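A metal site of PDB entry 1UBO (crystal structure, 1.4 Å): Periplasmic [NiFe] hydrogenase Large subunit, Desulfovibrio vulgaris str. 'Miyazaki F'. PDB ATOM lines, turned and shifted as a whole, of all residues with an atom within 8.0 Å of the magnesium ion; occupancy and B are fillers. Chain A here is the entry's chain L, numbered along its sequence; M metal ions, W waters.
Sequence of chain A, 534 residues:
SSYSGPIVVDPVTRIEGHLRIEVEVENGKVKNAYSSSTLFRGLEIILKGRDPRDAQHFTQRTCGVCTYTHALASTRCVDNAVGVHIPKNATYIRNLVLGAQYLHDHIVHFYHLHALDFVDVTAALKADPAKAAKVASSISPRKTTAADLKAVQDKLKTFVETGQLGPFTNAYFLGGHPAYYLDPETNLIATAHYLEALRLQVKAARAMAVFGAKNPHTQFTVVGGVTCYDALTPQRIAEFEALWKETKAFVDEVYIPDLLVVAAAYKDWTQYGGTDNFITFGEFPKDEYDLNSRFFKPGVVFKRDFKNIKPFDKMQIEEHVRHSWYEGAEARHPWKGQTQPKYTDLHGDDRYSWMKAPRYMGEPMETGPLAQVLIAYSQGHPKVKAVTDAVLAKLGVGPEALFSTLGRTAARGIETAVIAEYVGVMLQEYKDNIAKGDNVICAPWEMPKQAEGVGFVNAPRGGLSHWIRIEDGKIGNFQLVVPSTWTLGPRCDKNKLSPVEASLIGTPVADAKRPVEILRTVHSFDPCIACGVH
The side-chain amide oxygen (OE1) of Gln 479 lies close to the side-chain carboxylate (OE2) of Glu 44 (3.4 Å).
The side-chain carboxylate of Glu 44 is in salt-bridge range of the side-chain amino group of Lys 356, at 3.9 Å.
The side-chain carboxylate of Glu 44 sits at hydrogen-bond distance from the side-chain hydroxyl of Thr 339 (2.7 Å).
A ring nitrogen (ND1) of His 534 sits at hydrogen-bond distance from the backbone carbonyl oxygen (O) of Cys 531, 2.8 Å away.
Within 4 Å of the magnesium ion: Glu 44, Leu 480 and His 534.
The magnesium ion is bound by water W1 (2.1 Å), water W3 (2.1 Å), water W2 (2.1 Å), the side-chain carboxylate (OE2) of Glu 44 (2.1 Å), a ring nitrogen (NE2) of His 534 (2.2 Å) and the backbone carbonyl oxygen (O) of Leu 480 (2.2 Å).
Water W2 bridges the side-chain carboxylate (OE1) of Glu 44 (2.7 Å) and the side-chain amino group (NZ) of Lys 356 (3.0 Å).
Water W3 lies within hydrogen-bond range of OE2 of Glu 319 (2.5 Å), OE1 of Gln 479 (2.8 Å) and NZ of Lys 356 (3.1 Å).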
ATOM      1  N   PHE A  40     -19.264  30.224   8.326  1.00  0.00           N
ATOM      2  CA  PHE A  40     -19.021  29.685   9.647  1.00  0.00           C
ATOM      3  C   PHE A  40     -19.767  30.557  10.674  1.00  0.00           C
ATOM      4  O   PHE A  40     -19.764  31.805  10.557  1.00  0.00           O
ATOM      5  CB  PHE A  40     -17.503  29.706   9.913  1.00  0.00           C
ATOM      6  CG  PHE A  40     -17.123  29.241  11.305  1.00  0.00           C
ATOM      7  CD1 PHE A  40     -17.097  27.900  11.664  1.00  0.00           C
ATOM      8  CD2 PHE A  40     -16.780  30.164  12.298  1.00  0.00           C
ATOM      9  CE1 PHE A  40     -16.723  27.484  12.955  1.00  0.00           C
ATOM     10  CE2 PHE A  40     -16.407  29.748  13.565  1.00  0.00           C
ATOM     11  CZ  PHE A  40     -16.331  28.415  13.918  1.00  0.00           C
ATOM     12  N   GLU A  44     -20.368  25.781  18.466  1.00  0.00           N
ATOM     13  CA  GLU A  44     -19.632  24.990  19.456  1.00  0.00           C
ATOM     14  C   GLU A  44     -18.777  25.882  20.353  1.00  0.00           C
ATOM     15  O   GLU A  44     -18.634  25.631  21.548  1.00  0.00           O
ATOM     16  CB  GLU A  44     -18.762  23.928  18.765  1.00  0.00           C
ATOM     17  CG  GLU A  44     -19.607  22.811  18.088  1.00  0.00           C
ATOM     18  CD  GLU A  44     -18.879  22.216  16.891  1.00  0.00           C
ATOM     19  OE1 GLU A  44     -17.901  22.823  16.381  1.00  0.00           O
ATOM     20  OE2 GLU A  44     -19.350  21.139  16.451  1.00  0.00           O
ATOM     21  N   GLU A 319     -13.187  13.589  13.190  1.00  0.00           N
ATOM     22  CA  GLU A 319     -13.393  14.727  12.270  1.00  0.00           C
ATOM     23  C   GLU A 319     -12.066  15.377  11.888  1.00  0.00           C
ATOM     24  O   GLU A 319     -11.346  15.852  12.774  1.00  0.00           O
ATOM     25  CB  GLU A 319     -14.331  15.785  12.869  1.00  0.00           C
ATOM     26  CG  GLU A 319     -15.736  15.202  13.113  1.00  0.00           C
ATOM     27  CD  GLU A 319     -16.621  16.355  13.585  1.00  0.00           C
ATOM     28  OE1 GLU A 319     -17.442  16.833  12.736  1.00  0.00           O
ATOM     29  OE2 GLU A 319     -16.485  16.784  14.732  1.00  0.00           O
ATOM     30  N   TYR A 326      -9.460  25.292   9.735  1.00  0.00           N
ATOM     31  CA  TYR A 326      -9.254  25.171  11.176  1.00  0.00           C
ATOM     32  C   TYR A 326      -7.762  24.980  11.435  1.00  0.00           C
ATOM     33  O   TYR A 326      -7.025  24.617  10.508  1.00  0.00           O
ATOM     34  CB  TYR A 326     -10.048  23.990  11.841  1.00  0.00           C
ATOM     35  CG  TYR A 326     -11.521  24.213  11.631  1.00  0.00           C
ATOM     36  CD1 TYR A 326     -12.204  23.563  10.593  1.00  0.00           C
ATOM     37  CD2 TYR A 326     -12.233  25.074  12.476  1.00  0.00           C
ATOM     38  CE1 TYR A 326     -13.564  23.777  10.404  1.00  0.00           C
ATOM     39  CE2 TYR A 326     -13.598  25.299  12.283  1.00  0.00           C
ATOM     40  CZ  TYR A 326     -14.268  24.642  11.253  1.00  0.00           C
ATOM     41  OH  TYR A 326     -15.611  24.877  11.055  1.00  0.00           O
ATOM     42  N   PRO A 334     -15.162  13.373  18.506  1.00  0.00           N
ATOM     43  CA  PRO A 334     -15.874  14.546  19.022  1.00  0.00           C
ATOM     44  C   PRO A 334     -15.885  14.663  20.556  1.00  0.00           C
ATOM     45  O   PRO A 334     -16.090  15.804  21.013  1.00  0.00           O
ATOM     46  CB  PRO A 334     -17.300  14.376  18.489  1.00  0.00           C
ATOM     47  CG  PRO A 334     -17.349  13.164  17.676  1.00  0.00           C
ATOM     48  CD  PRO A 334     -16.013  12.521  17.650  1.00  0.00           C
ATOM     49  N   GLY A 337     -13.153  16.905  20.668  1.00  0.00           N
ATOM     50  CA  GLY A 337     -13.220  17.780  19.509  1.00  0.00           C
ATOM     51  C   GLY A 337     -12.611  19.138  19.749  1.00  0.00           C
ATOM     52  O   GLY A 337     -12.464  19.613  20.893  1.00  0.00           O
ATOM     53  N   GLN A 338     -12.256  19.779  18.629  1.00  0.00           N
ATOM     54  CA  GLN A 338     -11.691  21.126  18.686  1.00  0.00           C
ATOM     55  C   GLN A 338     -12.293  21.960  17.558  1.00  0.00           C
ATOM     56  O   GLN A 338     -12.437  21.427  16.434  1.00  0.00           O
ATOM     57  CB  GLN A 338     -10.178  21.138  18.462  1.00  0.00           C
ATOM     58  CG  GLN A 338      -9.405  20.342  19.536  1.00  0.00           C
ATOM     59  CD  GLN A 338      -7.913  20.373  19.275  1.00  0.00           C
ATOM     60  OE1 GLN A 338      -7.133  20.838  20.106  1.00  0.00           O
ATOM     61  NE2 GLN A 338      -7.545  19.866  18.109  1.00  0.00           N
ATOM     62  N   THR A 339     -12.622  23.201  17.874  1.00  0.00           N
ATOM     63  CA  THR A 339     -13.182  24.071  16.822  1.00  0.00           C
ATOM     64  C   THR A 339     -12.421  25.384  16.872  1.00  0.00           C
ATOM     65  O   THR A 339     -12.768  26.312  17.628  1.00  0.00           O
ATOM     66  CB  THR A 339     -14.693  24.251  17.026  1.00  0.00           C
ATOM     67  OG1 THR A 339     -15.254  22.926  17.034  1.00  0.00           O
ATOM     68  CG2 THR A 339     -15.327  25.047  15.882  1.00  0.00           C
ATOM     69  N   TRP A 354     -15.390  25.412   5.394  1.00  0.00           N
ATOM     70  CA  TRP A 354     -15.623  25.550   6.827  1.00  0.00           C
ATOM     71  C   TRP A 354     -16.174  24.261   7.432  1.00  0.00           C
ATOM     72  O   TRP A 354     -16.292  24.166   8.684  1.00  0.00           O
ATOM     73  CB  TRP A 354     -16.600  26.696   7.131  1.00  0.00           C
ATOM     74  CG  TRP A 354     -15.964  28.046   6.969  1.00  0.00           C
ATOM     75  CD1 TRP A 354     -16.234  28.965   5.998  1.00  0.00           C
ATOM     76  CD2 TRP A 354     -14.938  28.647   7.782  1.00  0.00           C
ATOM     77  NE1 TRP A 354     -15.462  30.101   6.155  1.00  0.00           N
ATOM     78  CE2 TRP A 354     -14.656  29.928   7.251  1.00  0.00           C
ATOM     79  CE3 TRP A 354     -14.260  28.200   8.922  1.00  0.00           C
ATOM     80  CZ2 TRP A 354     -13.682  30.757   7.845  1.00  0.00           C
ATOM     81  CZ3 TRP A 354     -13.308  29.036   9.496  1.00  0.00           C
ATOM     82  CH2 TRP A 354     -13.042  30.296   8.950  1.00  0.00           C
ATOM     83  N   MET A 355     -16.524  23.260   6.629  1.00  0.00           N
ATOM     84  CA  MET A 355     -16.896  21.979   7.232  1.00  0.00           C
ATOM     85  C   MET A 355     -15.652  21.177   7.595  1.00  0.00           C
ATOM     86  O   MET A 355     -14.643  21.152   6.873  1.00  0.00           O
ATOM     87  CB  MET A 355     -17.715  21.120   6.273  1.00  0.00           C
ATOM     88  CG  MET A 355     -19.162  21.624   6.108  1.00  0.00           C
ATOM     89  SD  MET A 355     -20.102  20.262   5.349  1.00  0.00           S
ATOM     90  CE  MET A 355     -21.479  21.157   4.641  1.00  0.00           C
ATOM     91  N   LYS A 356     -15.726  20.476   8.753  1.00  0.00           N
ATOM     92  CA  LYS A 356     -14.770  19.404   9.060  1.00  0.00           C
ATOM     93  C   LYS A 356     -15.096  18.228   8.180  1.00  0.00           C
ATOM     94  O   LYS A 356     -16.150  18.213   7.535  1.00  0.00           O
ATOM     95  CB  LYS A 356     -14.880  18.991  10.527  1.00  0.00           C
ATOM     96  CG  LYS A 356     -14.576  20.133  11.493  1.00  0.00           C
ATOM     97  CD  LYS A 356     -14.757  19.715  12.955  1.00  0.00           C
ATOM     98  CE  LYS A 356     -14.422  20.889  13.896  1.00  0.00           C
ATOM     99  NZ  LYS A 356     -14.886  20.526  15.278  1.00  0.00           N
ATOM    100  N   PRO A 358     -15.697  14.391   8.533  1.00  0.00           N
ATOM    101  CA  PRO A 358     -15.825  13.202   9.382  1.00  0.00           C
ATOM    102  C   PRO A 358     -15.479  11.943   8.596  1.00  0.00           C
ATOM    103  O   PRO A 358     -15.834  11.788   7.421  1.00  0.00           O
ATOM    104  CB  PRO A 358     -17.309  13.203   9.765  1.00  0.00           C
ATOM    105  CG  PRO A 358     -17.806  14.590   9.428  1.00  0.00           C
ATOM    106  CD  PRO A 358     -16.995  14.967   8.188  1.00  0.00           C
ATOM    107  N   SER A 465     -25.168  13.532  15.449  1.00  0.00           N
ATOM    108  CA  SER A 465     -24.788  13.229  16.836  1.00  0.00           C
ATOM    109  C   SER A 465     -24.306  14.516  17.491  1.00  0.00           C
ATOM    110  O   SER A 465     -23.611  15.334  16.881  1.00  0.00           O
ATOM    111  CB  SER A 465     -23.733  12.105  16.884  1.00  0.00           C
ATOM    112  OG  SER A 465     -22.614  12.334  16.053  1.00  0.00           O
ATOM    113  N   TRP A 467     -22.410  15.752  21.144  1.00  0.00           N
ATOM    114  CA  TRP A 467     -21.491  15.137  22.106  1.00  0.00           C
ATOM    115  C   TRP A 467     -21.130  16.150  23.178  1.00  0.00           C
ATOM    116  O   TRP A 467     -20.663  17.262  22.838  1.00  0.00           O
ATOM    117  CB  TRP A 467     -20.234  14.709  21.368  1.00  0.00           C
ATOM    118  CG  TRP A 467     -20.432  13.816  20.178  1.00  0.00           C
ATOM    119  CD1 TRP A 467     -20.886  14.100  18.937  1.00  0.00           C
ATOM    120  CD2 TRP A 467     -20.141  12.400  20.191  1.00  0.00           C
ATOM    121  NE1 TRP A 467     -20.893  12.941  18.176  1.00  0.00           N
ATOM    122  CE2 TRP A 467     -20.438  11.894  18.922  1.00  0.00           C
ATOM    123  CE3 TRP A 467     -19.649  11.514  21.167  1.00  0.00           C
ATOM    124  CZ2 TRP A 467     -20.268  10.546  18.573  1.00  0.00           C
ATOM    125  CZ3 TRP A 467     -19.470  10.182  20.855  1.00  0.00           C
ATOM    126  CH2 TRP A 467     -19.792   9.713  19.563  1.00  0.00           C
ATOM    127  N   PHE A 478     -18.690  20.864  23.651  1.00  0.00           N
ATOM    128  CA  PHE A 478     -19.929  20.442  23.000  1.00  0.00           C
ATOM    129  C   PHE A 478     -19.615  20.350  21.504  1.00  0.00           C
ATOM    130  O   PHE A 478     -19.185  21.376  20.964  1.00  0.00           O
ATOM    131  CB  PHE A 478     -21.070  21.423  23.279  1.00  0.00           C
ATOM    132  CG  PHE A 478     -22.441  20.763  23.070  1.00  0.00           C
ATOM    133  CD1 PHE A 478     -22.894  20.520  21.766  1.00  0.00           C
ATOM    134  CD2 PHE A 478     -23.238  20.387  24.125  1.00  0.00           C
ATOM    135  CE1 PHE A 478     -24.111  19.898  21.589  1.00  0.00           C
ATOM    136  CE2 PHE A 478     -24.483  19.779  23.933  1.00  0.00           C
ATOM    137  CZ  PHE A 478     -24.966  19.498  22.637  1.00  0.00           C
ATOM    138  N   GLN A 479     -19.795  19.175  20.926  1.00  0.00           N
ATOM    139  CA  GLN A 479     -19.433  19.031  19.505  1.00  0.00           C
ATOM    140  C   GLN A 479     -20.644  18.487  18.753  1.00  0.00           C
ATOM    141  O   GLN A 479     -21.236  17.517  19.206  1.00  0.00           O
ATOM    142  CB  GLN A 479     -18.218  18.111  19.360  1.00  0.00           C
ATOM    143  CG  GLN A 479     -16.919  18.686  19.925  1.00  0.00           C
ATOM    144  CD  GLN A 479     -16.400  19.870  19.107  1.00  0.00           C
ATOM    145  OE1 GLN A 479     -16.516  19.875  17.869  1.00  0.00           O
ATOM    146  NE2 GLN A 479     -15.789  20.821  19.793  1.00  0.00           N
ATOM    147  N   LEU A 480     -20.981  19.101  17.620  1.00  0.00           N
ATOM    148  CA  LEU A 480     -21.988  18.611  16.678  1.00  0.00           C
ATOM    149  C   LEU A 480     -21.300  17.943  15.502  1.00  0.00           C
ATOM    150  O   LEU A 480     -20.362  18.501  14.981  1.00  0.00           O
ATOM    151  CB  LEU A 480     -22.868  19.744  16.145  1.00  0.00           C
ATOM    152  CG  LEU A 480     -23.575  20.695  17.119  1.00  0.00           C
ATOM    153  CD1 LEU A 480     -24.757  21.312  16.363  1.00  0.00           C
ATOM    154  CD2 LEU A 480     -24.042  20.027  18.341  1.00  0.00           C
ATOM    155  N   VAL A 481     -21.729  16.733  15.153  1.00  0.00           N
ATOM    156  CA  VAL A 481     -21.220  16.064  13.946  1.00  0.00           C
ATOM    157  C   VAL A 481     -22.506  15.810  13.169  1.00  0.00           C
ATOM    158  O   VAL A 481     -23.343  15.047  13.631  1.00  0.00           O
ATOM    159  CB  VAL A 481     -20.499  14.757  14.224  1.00  0.00           C
ATOM    160  CG1 VAL A 481     -19.907  14.180  12.914  1.00  0.00           C
ATOM    161  CG2 VAL A 481     -19.412  14.978  15.256  1.00  0.00           C
ATOM    162  N   VAL A 482     -22.681  16.485  12.048  1.00  0.00           N
ATOM    163  CA  VAL A 482     -24.022  16.581  11.463  1.00  0.00           C
ATOM    164  C   VAL A 482     -24.077  15.852  10.137  1.00  0.00           C
ATOM    165  O   VAL A 482     -23.022  15.678   9.492  1.00  0.00           O
ATOM    166  CB  VAL A 482     -24.330  18.087  11.366  1.00  0.00           C
ATOM    167  CG1 VAL A 482     -25.722  18.377  10.885  1.00  0.00           C
ATOM    168  CG2 VAL A 482     -24.163  18.783  12.721  1.00  0.00           C
ATOM    169  N   THR A 485     -22.234  17.271   7.307  1.00  0.00           N
ATOM    170  CA  THR A 485     -20.806  17.271   7.518  1.00  0.00           C
ATOM    171  C   THR A 485     -20.205  16.011   6.898  1.00  0.00           C
ATOM    172  O   THR A 485     -19.187  16.090   6.202  1.00  0.00           O
ATOM    173  CB  THR A 485     -20.454  17.334   9.023  1.00  0.00           C
ATOM    174  OG1 THR A 485     -21.354  18.213   9.728  1.00  0.00           O
ATOM    175  CG2 THR A 485     -19.046  17.859   9.183  1.00  0.00           C
ATOM    176  N   CYS A 531     -26.249  23.344   8.877  1.00  0.00           N
ATOM    177  CA  CYS A 531     -26.049  22.077   9.541  1.00  0.00           C
ATOM    178  C   CYS A 531     -24.591  21.627   9.486  1.00  0.00           C
ATOM    179  O   CYS A 531     -23.990  21.252  10.504  1.00  0.00           O
ATOM    180  CB  CYS A 531     -26.920  20.973   8.923  1.00  0.00           C
ATOM    181  SG  CYS A 531     -28.527  20.845   9.741  1.00  0.00           S
ATOM    182  N   GLY A 532     -24.021  21.589   8.285  1.00  0.00           N
ATOM    183  CA  GLY A 532     -22.726  20.917   8.174  1.00  0.00           C
ATOM    184  C   GLY A 532     -21.622  21.639   8.904  1.00  0.00           C
ATOM    185  O   GLY A 532     -20.707  20.990   9.432  1.00  0.00           O
ATOM    186  N   VAL A 533     -21.712  22.974   8.935  1.00  0.00           N
ATOM    187  CA  VAL A 533     -20.667  23.790   9.559  1.00  0.00           C
ATOM    188  C   VAL A 533     -20.959  24.252  10.966  1.00  0.00           C
ATOM    189  O   VAL A 533     -20.086  24.210  11.838  1.00  0.00           O
ATOM    190  CB  VAL A 533     -20.406  25.100   8.776  1.00  0.00           C
ATOM    191  CG1 VAL A 533     -19.339  25.971   9.465  1.00  0.00           C
ATOM    192  CG2 VAL A 533     -19.996  24.779   7.338  1.00  0.00           C
ATOM    193  N   HIS A 534     -22.205  24.674  11.255  1.00  0.00           N
ATOM    194  CA  HIS A 534     -22.586  25.191  12.613  1.00  0.00           C
ATOM    195  C   HIS A 534     -21.551  26.165  13.179  1.00  0.00           C
ATOM    196  O   HIS A 534     -21.136  27.081  12.298  1.00  0.00           O
ATOM    197  CB  HIS A 534     -22.949  24.101  13.616  1.00  0.00           C
ATOM    198  CG  HIS A 534     -22.110  22.863  13.625  1.00  0.00           C
ATOM    199  ND1 HIS A 534     -22.244  21.892  12.640  1.00  0.00           N
ATOM    200  CD2 HIS A 534     -21.048  22.516  14.366  1.00  0.00           C
ATOM    201  CE1 HIS A 534     -21.327  20.993  12.849  1.00  0.00           C
ATOM    202  NE2 HIS A 534     -20.591  21.324  13.916  1.00  0.00           N
ATOM    203  OXT HIS A 534     -21.190  26.175  14.298  1.00  0.00           O
HETATM  204 MG    MG M   1     -18.965  20.107  14.630  1.00  0.00          MG
HETATM  205  O   HOH W   1     -18.518  19.226  12.821  1.00  0.00           O
HETATM  206  O   HOH W   2     -17.511  21.490  14.068  1.00  0.00           O
HETATM  207  O   HOH W   3     -17.517  18.908  15.489  1.00  0.00           O
